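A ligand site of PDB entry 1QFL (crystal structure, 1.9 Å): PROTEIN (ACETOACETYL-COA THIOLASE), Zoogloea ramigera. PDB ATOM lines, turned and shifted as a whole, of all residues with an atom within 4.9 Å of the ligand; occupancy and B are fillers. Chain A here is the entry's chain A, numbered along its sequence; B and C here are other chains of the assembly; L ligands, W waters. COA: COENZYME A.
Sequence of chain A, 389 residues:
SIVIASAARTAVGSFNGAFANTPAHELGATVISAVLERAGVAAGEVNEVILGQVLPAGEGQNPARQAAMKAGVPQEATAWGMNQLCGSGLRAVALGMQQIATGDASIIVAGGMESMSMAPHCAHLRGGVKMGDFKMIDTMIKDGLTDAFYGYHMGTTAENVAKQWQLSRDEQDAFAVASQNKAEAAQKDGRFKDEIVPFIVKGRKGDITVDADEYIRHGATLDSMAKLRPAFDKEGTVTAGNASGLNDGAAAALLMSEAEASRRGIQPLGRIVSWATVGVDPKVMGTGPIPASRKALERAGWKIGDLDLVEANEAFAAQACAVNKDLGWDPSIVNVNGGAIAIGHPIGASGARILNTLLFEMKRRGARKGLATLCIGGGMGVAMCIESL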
ATOM      1  N   SCY A  86       1.500  27.362   7.951  1.00  0.00           N
ATOM      2  CA  SCY A  86       2.833  27.361   7.380  1.00  0.00           C
ATOM      3  CB  SCY A  86       2.917  26.350   6.152  1.00  0.00           C
ATOM      4  SG  SCY A  86       2.602  24.744   6.894  1.00  0.00           S
ATOM      5  CD  SCY A  86       0.969  24.503   6.104  1.00  0.00           C
ATOM      6  OCD SCY A  86       0.942  24.286   4.922  1.00  0.00           O
ATOM      7  CE  SCY A  86      -0.328  24.571   6.928  1.00  0.00           C
ATOM      8  C   SCY A  86       3.253  28.692   6.836  1.00  0.00           C
ATOM      9  O   SCY A  86       4.438  28.919   6.633  1.00  0.00           O
ATOM     10  N   LEU A 145      -1.801  19.929  11.207  1.00  0.00           N
ATOM     11  CA  LEU A 145      -1.806  19.248   9.946  1.00  0.00           C
ATOM     12  C   LEU A 145      -3.097  18.713   9.383  1.00  0.00           C
ATOM     13  O   LEU A 145      -3.180  18.069   8.291  1.00  0.00           O
ATOM     14  CB  LEU A 145      -0.785  18.097  10.066  1.00  0.00           C
ATOM     15  CG  LEU A 145       0.587  18.367  10.693  1.00  0.00           C
ATOM     16  CD1 LEU A 145       1.370  17.072  10.924  1.00  0.00           C
ATOM     17  CD2 LEU A 145       1.351  19.379   9.837  1.00  0.00           C
ATOM     18  N   HIS A 153      -5.891  14.762   6.355  1.00  0.00           N
ATOM     19  CA  HIS A 153      -4.550  15.395   6.485  1.00  0.00           C
ATOM     20  C   HIS A 153      -4.204  16.329   5.355  1.00  0.00           C
ATOM     21  O   HIS A 153      -4.705  16.224   4.248  1.00  0.00           O
ATOM     22  CB  HIS A 153      -3.489  14.278   6.553  1.00  0.00           C
ATOM     23  CG  HIS A 153      -2.143  14.671   7.063  1.00  0.00           C
ATOM     24  ND1 HIS A 153      -1.216  15.354   6.303  1.00  0.00           N
ATOM     25  CD2 HIS A 153      -1.530  14.418   8.244  1.00  0.00           C
ATOM     26  CE1 HIS A 153      -0.085  15.519   7.008  1.00  0.00           C
ATOM     27  NE2 HIS A 153      -0.250  14.918   8.203  1.00  0.00           N
ATOM     28  N   MET A 154      -3.219  17.205   5.597  1.00  0.00           N
ATOM     29  CA  MET A 154      -2.666  18.111   4.579  1.00  0.00           C
ATOM     30  C   MET A 154      -2.188  17.269   3.387  1.00  0.00           C
ATOM     31  O   MET A 154      -2.236  17.679   2.227  1.00  0.00           O
ATOM     32  CB  MET A 154      -1.503  18.889   5.190  1.00  0.00           C
ATOM     33  CG  MET A 154      -1.921  20.004   6.161  1.00  0.00           C
ATOM     34  SD  MET A 154      -2.957  21.226   5.296  1.00  0.00           S
ATOM     35  CE  MET A 154      -4.601  20.890   5.863  1.00  0.00           C
ATOM     36  N   GLY A 155      -1.740  16.028   3.666  1.00  0.00           N
ATOM     37  CA  GLY A 155      -1.285  15.160   2.568  1.00  0.00           C
ATOM     38  C   GLY A 155      -2.377  14.715   1.599  1.00  0.00           C
ATOM     39  O   GLY A 155      -2.101  14.329   0.467  1.00  0.00           O
ATOM     40  N   GLN A 180      16.629  16.306  -2.168  1.00  0.00           N
ATOM     41  CA  GLN A 180      17.617  15.718  -1.298  1.00  0.00           C
ATOM     42  C   GLN A 180      19.025  15.922  -1.854  1.00  0.00           C
ATOM     43  O   GLN A 180      19.874  16.397  -1.105  1.00  0.00           O
ATOM     44  CB  GLN A 180      17.399  14.185  -1.144  1.00  0.00           C
ATOM     45  CG  GLN A 180      16.046  13.930  -0.498  1.00  0.00           C
ATOM     46  CD  GLN A 180      16.171  14.109   1.012  1.00  0.00           C
ATOM     47  OE1 GLN A 180      17.202  14.531   1.551  1.00  0.00           O
ATOM     48  NE2 GLN A 180      15.072  13.778   1.674  1.00  0.00           N
ATOM     49  N   ARG A 217      18.800  13.793   3.785  1.00  0.00           N
ATOM     50  CA  ARG A 217      19.366  12.453   3.610  1.00  0.00           C
ATOM     51  C   ARG A 217      20.528  12.448   2.613  1.00  0.00           C
ATOM     52  O   ARG A 217      20.498  12.984   1.475  1.00  0.00           O
ATOM     53  CB  ARG A 217      18.471  11.271   3.422  1.00  0.00           C
ATOM     54  CG  ARG A 217      17.099  11.458   2.868  1.00  0.00           C
ATOM     55  CD  ARG A 217      16.029  10.682   3.567  1.00  0.00           C
ATOM     56  NE  ARG A 217      16.198   9.259   3.445  1.00  0.00           N
ATOM     57  CZ  ARG A 217      15.678   8.372   4.281  1.00  0.00           C
ATOM     58  NH1 ARG A 217      14.920   8.680   5.330  1.00  0.00           N
ATOM     59  NH2 ARG A 217      15.991   7.118   4.004  1.00  0.00           N
ATOM     60  N   SER A 224      14.828   3.435  -3.624  1.00  0.00           N
ATOM     61  CA  SER A 224      14.181   3.268  -2.320  1.00  0.00           C
ATOM     62  C   SER A 224      12.999   4.230  -2.159  1.00  0.00           C
ATOM     63  O   SER A 224      12.088   4.000  -1.391  1.00  0.00           O
ATOM     64  CB  SER A 224      15.188   3.507  -1.205  1.00  0.00           C
ATOM     65  OG  SER A 224      15.433   4.927  -1.328  1.00  0.00           O
ATOM     66  N   MET A 225      12.996   5.331  -2.879  1.00  0.00           N
ATOM     67  CA  MET A 225      11.888   6.304  -2.823  1.00  0.00           C
ATOM     68  C   MET A 225      10.672   5.649  -3.497  1.00  0.00           C
ATOM     69  O   MET A 225       9.483   5.638  -3.116  1.00  0.00           O
ATOM     70  CB  MET A 225      12.469   7.455  -3.563  1.00  0.00           C
ATOM     71  CG  MET A 225      12.016   8.747  -4.103  1.00  0.00           C
ATOM     72  SD  MET A 225      12.243   9.976  -2.711  1.00  0.00           S
ATOM     73  CE  MET A 225      10.630   9.592  -2.264  1.00  0.00           C
ATOM     74  N   LEU A 228       8.469   3.128  -1.575  1.00  0.00           N
ATOM     75  CA  LEU A 228       7.707   3.484  -0.380  1.00  0.00           C
ATOM     76  C   LEU A 228       6.211   3.368  -0.621  1.00  0.00           C
ATOM     77  O   LEU A 228       5.816   3.518  -1.762  1.00  0.00           O
ATOM     78  CB  LEU A 228       8.046   4.921   0.071  1.00  0.00           C
ATOM     79  CG  LEU A 228       9.498   5.064   0.534  1.00  0.00           C
ATOM     80  CD1 LEU A 228       9.834   6.553   0.621  1.00  0.00           C
ATOM     81  CD2 LEU A 228       9.711   4.322   1.849  1.00  0.00           C
ATOM     82  N   ALA A 231       1.254   7.256   1.932  1.00  0.00           N
ATOM     83  CA  ALA A 231       1.040   7.464   3.343  1.00  0.00           C
ATOM     84  C   ALA A 231      -0.345   7.977   3.698  1.00  0.00           C
ATOM     85  O   ALA A 231      -0.632   7.822   4.873  1.00  0.00           O
ATOM     86  CB  ALA A 231       2.171   8.448   3.776  1.00  0.00           C
ATOM     87  N   PHE A 232      -1.117   8.576   2.804  1.00  0.00           N
ATOM     88  CA  PHE A 232      -2.410   9.136   3.186  1.00  0.00           C
ATOM     89  C   PHE A 232      -3.586   8.525   2.456  1.00  0.00           C
ATOM     90  O   PHE A 232      -4.698   8.408   2.960  1.00  0.00           O
ATOM     91  CB  PHE A 232      -2.393  10.669   2.936  1.00  0.00           C
ATOM     92  CG  PHE A 232      -1.259  11.360   3.652  1.00  0.00           C
ATOM     93  CD1 PHE A 232      -1.344  11.773   4.968  1.00  0.00           C
ATOM     94  CD2 PHE A 232      -0.070  11.626   2.942  1.00  0.00           C
ATOM     95  CE1 PHE A 232      -0.267  12.388   5.596  1.00  0.00           C
ATOM     96  CE2 PHE A 232       1.016  12.219   3.572  1.00  0.00           C
ATOM     97  CZ  PHE A 232       0.918  12.620   4.905  1.00  0.00           C
ATOM     98  N   THR A 239       3.968   9.923  -0.520  1.00  0.00           N
ATOM     99  CA  THR A 239       4.544   8.979   0.407  1.00  0.00           C
ATOM    100  C   THR A 239       5.364   9.752   1.433  1.00  0.00           C
ATOM    101  O   THR A 239       5.440  10.949   1.218  1.00  0.00           O
ATOM    102  CB  THR A 239       5.537   8.025  -0.349  1.00  0.00           C
ATOM    103  OG1 THR A 239       6.733   8.769  -0.616  1.00  0.00           O
ATOM    104  CG2 THR A 239       4.929   7.495  -1.626  1.00  0.00           C
ATOM    105  N   ALA A 240       6.019   9.030   2.366  1.00  0.00           N
ATOM    106  CA  ALA A 240       6.834   9.783   3.335  1.00  0.00           C
ATOM    107  C   ALA A 240       8.094  10.337   2.662  1.00  0.00           C
ATOM    108  O   ALA A 240       8.743  11.271   3.123  1.00  0.00           O
ATOM    109  CB  ALA A 240       7.269   8.897   4.472  1.00  0.00           C
ATOM    110  N   GLY A 241       8.479   9.704   1.551  1.00  0.00           N
ATOM    111  CA  GLY A 241       9.601  10.172   0.790  1.00  0.00           C
ATOM    112  C   GLY A 241       9.347  11.459   0.026  1.00  0.00           C
ATOM    113  O   GLY A 241      10.299  12.222  -0.212  1.00  0.00           O
ATOM    114  N   ALA A 243       7.018  13.879   0.644  1.00  0.00           N
ATOM    115  CA  ALA A 243       6.336  14.819   1.500  1.00  0.00           C
ATOM    116  C   ALA A 243       7.364  15.497   2.412  1.00  0.00           C
ATOM    117  O   ALA A 243       8.397  14.837   2.690  1.00  0.00           O
ATOM    118  CB  ALA A 243       5.292  14.204   2.431  1.00  0.00           C
ATOM    119  N   SER A 244       7.024  16.641   3.003  1.00  0.00           N
ATOM    120  CA  SER A 244       7.972  17.330   3.914  1.00  0.00           C
ATOM    121  C   SER A 244       7.994  16.518   5.174  1.00  0.00           C
ATOM    122  O   SER A 244       7.143  15.640   5.255  1.00  0.00           O
ATOM    123  CB  SER A 244       7.525  18.794   4.281  1.00  0.00           C
ATOM    124  OG  SER A 244       6.153  18.659   4.661  1.00  0.00           O
ATOM    125  N   GLY A 245       8.878  16.798   6.164  1.00  0.00           N
ATOM    126  CA  GLY A 245       8.761  15.923   7.358  1.00  0.00           C
ATOM    127  C   GLY A 245       8.095  16.782   8.445  1.00  0.00           C
ATOM    128  O   GLY A 245       7.646  17.934   8.275  1.00  0.00           O
ATOM    129  N   LEU A 246       8.129  16.248   9.629  1.00  0.00           N
ATOM    130  CA  LEU A 246       7.664  16.840  10.872  1.00  0.00           C
ATOM    131  C   LEU A 246       8.966  17.257  11.515  1.00  0.00           C
ATOM    132  O   LEU A 246       9.839  16.356  11.608  1.00  0.00           O
ATOM    133  CB  LEU A 246       7.005  15.695  11.684  1.00  0.00           C
ATOM    134  CG  LEU A 246       5.891  14.948  10.852  1.00  0.00           C
ATOM    135  CD1 LEU A 246       5.537  13.736  11.770  1.00  0.00           C
ATOM    136  CD2 LEU A 246       4.728  15.893  10.758  1.00  0.00           C
ATOM    137  N   MET A 285      -5.071  23.334  -1.078  1.00  0.00           N
ATOM    138  CA  MET A 285      -4.328  24.409  -0.379  1.00  0.00           C
ATOM    139  C   MET A 285      -2.913  24.637  -0.890  1.00  0.00           C
ATOM    140  O   MET A 285      -2.415  25.790  -0.864  1.00  0.00           O
ATOM    141  CB  MET A 285      -4.369  24.189   1.139  1.00  0.00           C
ATOM    142  CG  MET A 285      -3.540  22.997   1.649  1.00  0.00           C
ATOM    143  SD  MET A 285      -1.828  23.562   1.925  1.00  0.00           S
ATOM    144  CE  MET A 285      -0.941  22.016   1.880  1.00  0.00           C
ATOM    145  N   ALA A 315       6.001  21.757   0.715  1.00  0.00           N
ATOM    146  CA  ALA A 315       5.085  21.030   1.604  1.00  0.00           C
ATOM    147  C   ALA A 315       5.033  19.588   1.119  1.00  0.00           C
ATOM    148  O   ALA A 315       5.040  18.583   1.866  1.00  0.00           O
ATOM    149  CB  ALA A 315       3.672  21.660   1.522  1.00  0.00           C
ATOM    150  N   PHE A 316       4.845  19.424  -0.197  1.00  0.00           N
ATOM    151  CA  PHE A 316       4.753  18.066  -0.790  1.00  0.00           C
ATOM    152  C   PHE A 316       5.274  18.163  -2.192  1.00  0.00           C
ATOM    153  O   PHE A 316       5.020  19.206  -2.874  1.00  0.00           O
ATOM    154  CB  PHE A 316       3.274  17.552  -0.952  1.00  0.00           C
ATOM    155  CG  PHE A 316       2.633  17.410   0.397  1.00  0.00           C
ATOM    156  CD1 PHE A 316       2.781  16.229   1.115  1.00  0.00           C
ATOM    157  CD2 PHE A 316       1.926  18.451   0.951  1.00  0.00           C
ATOM    158  CE1 PHE A 316       2.232  16.115   2.397  1.00  0.00           C
ATOM    159  CE2 PHE A 316       1.377  18.351   2.236  1.00  0.00           C
ATOM    160  CZ  PHE A 316       1.538  17.186   2.947  1.00  0.00           C
ATOM    161  N   HIS A 345      10.374  20.604   7.795  1.00  0.00           N
ATOM    162  CA  HIS A 345       9.280  21.579   7.817  1.00  0.00           C
ATOM    163  C   HIS A 345       8.691  21.926   9.167  1.00  0.00           C
ATOM    164  O   HIS A 345       7.612  21.419   9.457  1.00  0.00           O
ATOM    165  CB  HIS A 345       8.092  20.928   6.993  1.00  0.00           C
ATOM    166  CG  HIS A 345       7.073  21.909   6.486  1.00  0.00           C
ATOM    167  ND1 HIS A 345       7.132  23.260   6.769  1.00  0.00           N
ATOM    168  CD2 HIS A 345       5.923  21.778   5.795  1.00  0.00           C
ATOM    169  CE1 HIS A 345       6.105  23.890   6.254  1.00  0.00           C
ATOM    170  NE2 HIS A 345       5.321  23.018   5.701  1.00  0.00           N
ATOM    171  N   ILE A 347       6.626  23.760  10.876  1.00  0.00           N
ATOM    172  CA  ILE A 347       5.583  24.641  10.413  1.00  0.00           C
ATOM    173  C   ILE A 347       5.629  26.107  10.711  1.00  0.00           C
ATOM    174  O   ILE A 347       5.648  26.871   9.746  1.00  0.00           O
ATOM    175  CB  ILE A 347       4.151  24.051  10.644  1.00  0.00           C
ATOM    176  CG1 ILE A 347       3.751  23.719  12.050  1.00  0.00           C
ATOM    177  CG2 ILE A 347       4.191  22.711   9.808  1.00  0.00           C
ATOM    178  CD1 ILE A 347       2.458  22.885  12.130  1.00  0.00           C
ATOM    179  N   CYS A 375       2.648  27.711   0.719  1.00  0.00           N
ATOM    180  CA  CYS A 375       1.294  27.220   0.715  1.00  0.00           C
ATOM    181  C   CYS A 375       0.810  27.153   2.159  1.00  0.00           C
ATOM    182  O   CYS A 375       1.647  26.989   3.064  1.00  0.00           O
ATOM    183  CB  CYS A 375       1.103  25.861   0.011  1.00  0.00           C
ATOM    184  SG  CYS A 375       1.722  24.413   0.916  1.00  0.00           S
ATOM    185  N   MET B 131       3.307   9.576  17.369  1.00  0.00           N
ATOM    186  CA  MET B 131       2.438  10.471  16.564  1.00  0.00           C
ATOM    187  C   MET B 131       1.036   9.858  16.534  1.00  0.00           C
ATOM    188  O   MET B 131       0.873   8.619  16.444  1.00  0.00           O
ATOM    189  CB  MET B 131       3.017  10.504  15.146  1.00  0.00           C
ATOM    190  CG  MET B 131       2.301  11.391  14.161  1.00  0.00           C
ATOM    191  SD  MET B 131       3.077  11.409  12.524  1.00  0.00           S
ATOM    192  CE  MET B 131       2.921   9.698  12.046  1.00  0.00           C
ATOM    193  N   LYS C 205       8.398  -7.679  12.066  1.00  0.00           N
ATOM    194  CA  LYS C 205       9.647  -7.604  11.320  1.00  0.00           C
ATOM    195  C   LYS C 205      10.579  -8.722  11.783  1.00  0.00           C
ATOM    196  O   LYS C 205      11.809  -8.647  11.693  1.00  0.00           O
ATOM    197  CB  LYS C 205      10.247  -6.207  11.501  1.00  0.00           C
ATOM    198  CG  LYS C 205       9.265  -5.054  11.395  1.00  0.00           C
ATOM    199  CD  LYS C 205       9.874  -3.726  10.959  1.00  0.00           C
ATOM    200  CE  LYS C 205       8.817  -2.680  10.643  1.00  0.00           C
ATOM    201  NZ  LYS C 205       9.331  -1.524   9.872  1.00  0.00           N
HETATM  202  N1A COA L   1      14.219   7.326   0.837  1.00  0.00           N
HETATM  203  C2A COA L   1      14.078   6.129   1.509  1.00  0.00           C
HETATM  204  N3A COA L   1      13.307   5.860   2.598  1.00  0.00           N
HETATM  205  C4A COA L   1      12.698   6.950   3.039  1.00  0.00           C
HETATM  206  C5A COA L   1      12.751   8.261   2.503  1.00  0.00           C
HETATM  207  C6A COA L   1      13.582   8.465   1.295  1.00  0.00           C
HETATM  208  N6A COA L   1      13.683   9.650   0.776  1.00  0.00           N
HETATM  209  N7A COA L   1      12.019   9.131   3.222  1.00  0.00           N
HETATM  210  C8A COA L   1      11.483   8.411   4.228  1.00  0.00           C
HETATM  211  N9A COA L   1      11.866   7.075   4.152  1.00  0.00           N
HETATM  212  C1B COA L   1      11.508   5.999   5.108  1.00  0.00           C
HETATM  213  C2B COA L   1      11.725   6.445   6.543  1.00  0.00           C
HETATM  214  O2B COA L   1      13.084   6.230   6.858  1.00  0.00           O
HETATM  215  C3B COA L   1      10.870   5.400   7.295  1.00  0.00           C
HETATM  216  O3B COA L   1      11.453   4.153   7.207  1.00  0.00           O
HETATM  217  P3B COA L   1      11.289   3.246   8.600  1.00  0.00           P
HETATM  218  O7A COA L   1      12.194   3.966   9.720  1.00  0.00           O
HETATM  219  O8A COA L   1       9.820   3.224   9.196  1.00  0.00           O
HETATM  220  O9A COA L   1      11.933   1.837   8.239  1.00  0.00           O
HETATM  221  C4B COA L   1       9.599   5.608   6.414  1.00  0.00           C
HETATM  222  O4B COA L   1      10.107   5.675   5.017  1.00  0.00           O
HETATM  223  C5B COA L   1       9.228   7.102   6.504  1.00  0.00           C
HETATM  224  O5B COA L   1       8.323   7.033   7.584  1.00  0.00           O
HETATM  225  P1A COA L   1       8.457   8.078   8.786  1.00  0.00           P
HETATM  226  O1A COA L   1       8.550   7.263  10.041  1.00  0.00           O
HETATM  227  O2A COA L   1       9.490   9.159   8.603  1.00  0.00           O
HETATM  228  O3A COA L   1       7.106   8.701   8.770  1.00  0.00           O
HETATM  229  P2A COA L   1       5.607   8.462   9.384  1.00  0.00           P
HETATM  230  O4A COA L   1       4.824   7.485   8.580  1.00  0.00           O
HETATM  231  O5A COA L   1       5.577   8.270  10.830  1.00  0.00           O
HETATM  232  O6A COA L   1       5.185  10.022   8.856  1.00  0.00           O
HETATM  233  CBP COA L   1       4.365  11.324   7.096  1.00  0.00           C
HETATM  234  CCP COA L   1       5.392  10.187   7.428  1.00  0.00           C
HETATM  235  CDP COA L   1       2.951  10.824   7.577  1.00  0.00           C
HETATM  236  CEP COA L   1       4.463  11.535   5.599  1.00  0.00           C
HETATM  237  CAP COA L   1       4.871  12.548   7.935  1.00  0.00           C
HETATM  238  OAP COA L   1       6.313  12.837   7.830  1.00  0.00           O
HETATM  239  C9P COA L   1       4.169  13.819   7.517  1.00  0.00           C
HETATM  240  O9P COA L   1       2.872  13.899   7.929  1.00  0.00           O
HETATM  241  N8P COA L   1       4.752  14.817   6.898  1.00  0.00           N
HETATM  242  C7P COA L   1       3.866  15.922   6.711  1.00  0.00           C
HETATM  243  C6P COA L   1       4.222  17.276   6.460  1.00  0.00           C
HETATM  244  C5P COA L   1       3.001  18.202   6.420  1.00  0.00           C
HETATM  245  O5P COA L   1       1.829  17.828   6.074  1.00  0.00           O
HETATM  246  N4P COA L   1       3.339  19.383   6.867  1.00  0.00           N
HETATM  247  C3P COA L   1       2.414  20.601   6.832  1.00  0.00           C
HETATM  248  C2P COA L   1       2.539  20.662   5.260  1.00  0.00           C
HETATM  249  S1P COA L   1       1.072  21.472   4.575  1.00  0.00           S
HETATM  250  O   HOH W   1       7.825  12.849   5.201  1.00  0.00           O
HETATM  251  O   HOH W   2      11.431  10.442   6.895  1.00  0.00           O
HETATM  252  O   HOH W   3      12.716  11.983   0.863  1.00  0.00           O
HETATM  253  O   HOH W   4      13.159   3.008   3.348  1.00  0.00           O
HETATM  254  O   HOH W   5       5.550  19.472   9.032  1.00  0.00           O
HETATM  255  O   HOH W   6      15.417   8.235  -1.162  1.00  0.00           O
HETATM  256  O   HOH W   7       1.459  13.221  10.034  1.00  0.00           O
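OCD of SCY 86 lies close to S1P of the ligand (2.8 Å). The backbone carbonyl oxygen of Ser 244 lies within hydrogen-bond range of a nitrogen (N8P) of the ligand (3.0 Å). NE2 of His 153 lies within hydrogen-bond range of O9P of the ligand (3.3 Å). NH2 of Arg 217 lies within hydrogen-bond range of N3A of the ligand (3.3 Å). OG of Ser 224 sits close to N1A of the ligand, 3.5 Å away. The side-chain sulfur (SD) of Met 225 lies within hydrogen-bond range of a nitrogen (N6A) of the ligand (3.8 Å).
A ring nitrogen (NE2) of His 345 sits at hydrogen-bond distance from SG of SCY 86, 3.4 Å away. N of Ser 244 lies within hydrogen-bond range of O of Ala 315 (3.0 Å). ND1 of His 153 sits at hydrogen-bond distance from N of Gly 155 (2.8 Å). OE1 of Gln 180 is in hydrogen-bond range of N of Arg 217 (2.8 Å). The side-chain sulfur of Met 285 lies close to the side-chain sulfur of Cys 375 (3.8 Å). The backbone carbonyl oxygen (O) of Leu 145 lies within hydrogen-bond range of the backbone NH (N) of Met 154. The backbone NH of Gly 241 is in hydrogen-bond range of the side-chain hydroxyl of Thr 239, 2.9 Å away.
Leu 145 touches the ligand. CB of Met 154 touches O5P of the ligand, at 3.6 Å. Leu 228 touches the ligand. CZ of Phe 232 touches CEP of the ligand (3.8 Å). CB of Ala 240 touches C5B of the ligand, at 3.3 Å. Gly 241 touches the ligand. Gly 245 touches the ligand (O to C6P, 3.9 Å). Leu 246 touches the ligand. CE of Met 285 touches S1P of the ligand, at 3.4 Å. Phe 316 touches the ligand (CZ to O5P, 3.2 Å). His 345 touches the ligand. CE of Met 131 of chain B touches O5A of the ligand (3.3 Å). 18 residues have an atom within 4 Å of the ligand: SCY 86, Leu 145, His 153, Met 154, Arg 217, Ser 224, Met 225, Leu 228, Phe 232, Ala 240, Gly 241, Ser 244, Gly 245, Leu 246, Met 285, Phe 316, His 345 and Met 131 of chain B. The nearest printed residue that does not touch the ligand is Ala 315 (4.01 Å).
Water W6 bridges N1A of the ligand and OG of Ser 224. Water W3 lies within hydrogen-bond range of N6A of the ligand (2.5 Å), O of Gly 241 (2.7 Å) and NE2 of Gln 180 (3.1 Å). Water W7 lies within hydrogen-bond range of O9P of the ligand (2.6 Å), NE2 of His 153 (3.0 Å) and SD of Met 131 of chain B (3.5 Å). Water W5 lies within hydrogen-bond range of O of Gly 245 (2.7 Å), O of His 345 (2.9 Å) and N4P of the ligand (3.1 Å).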
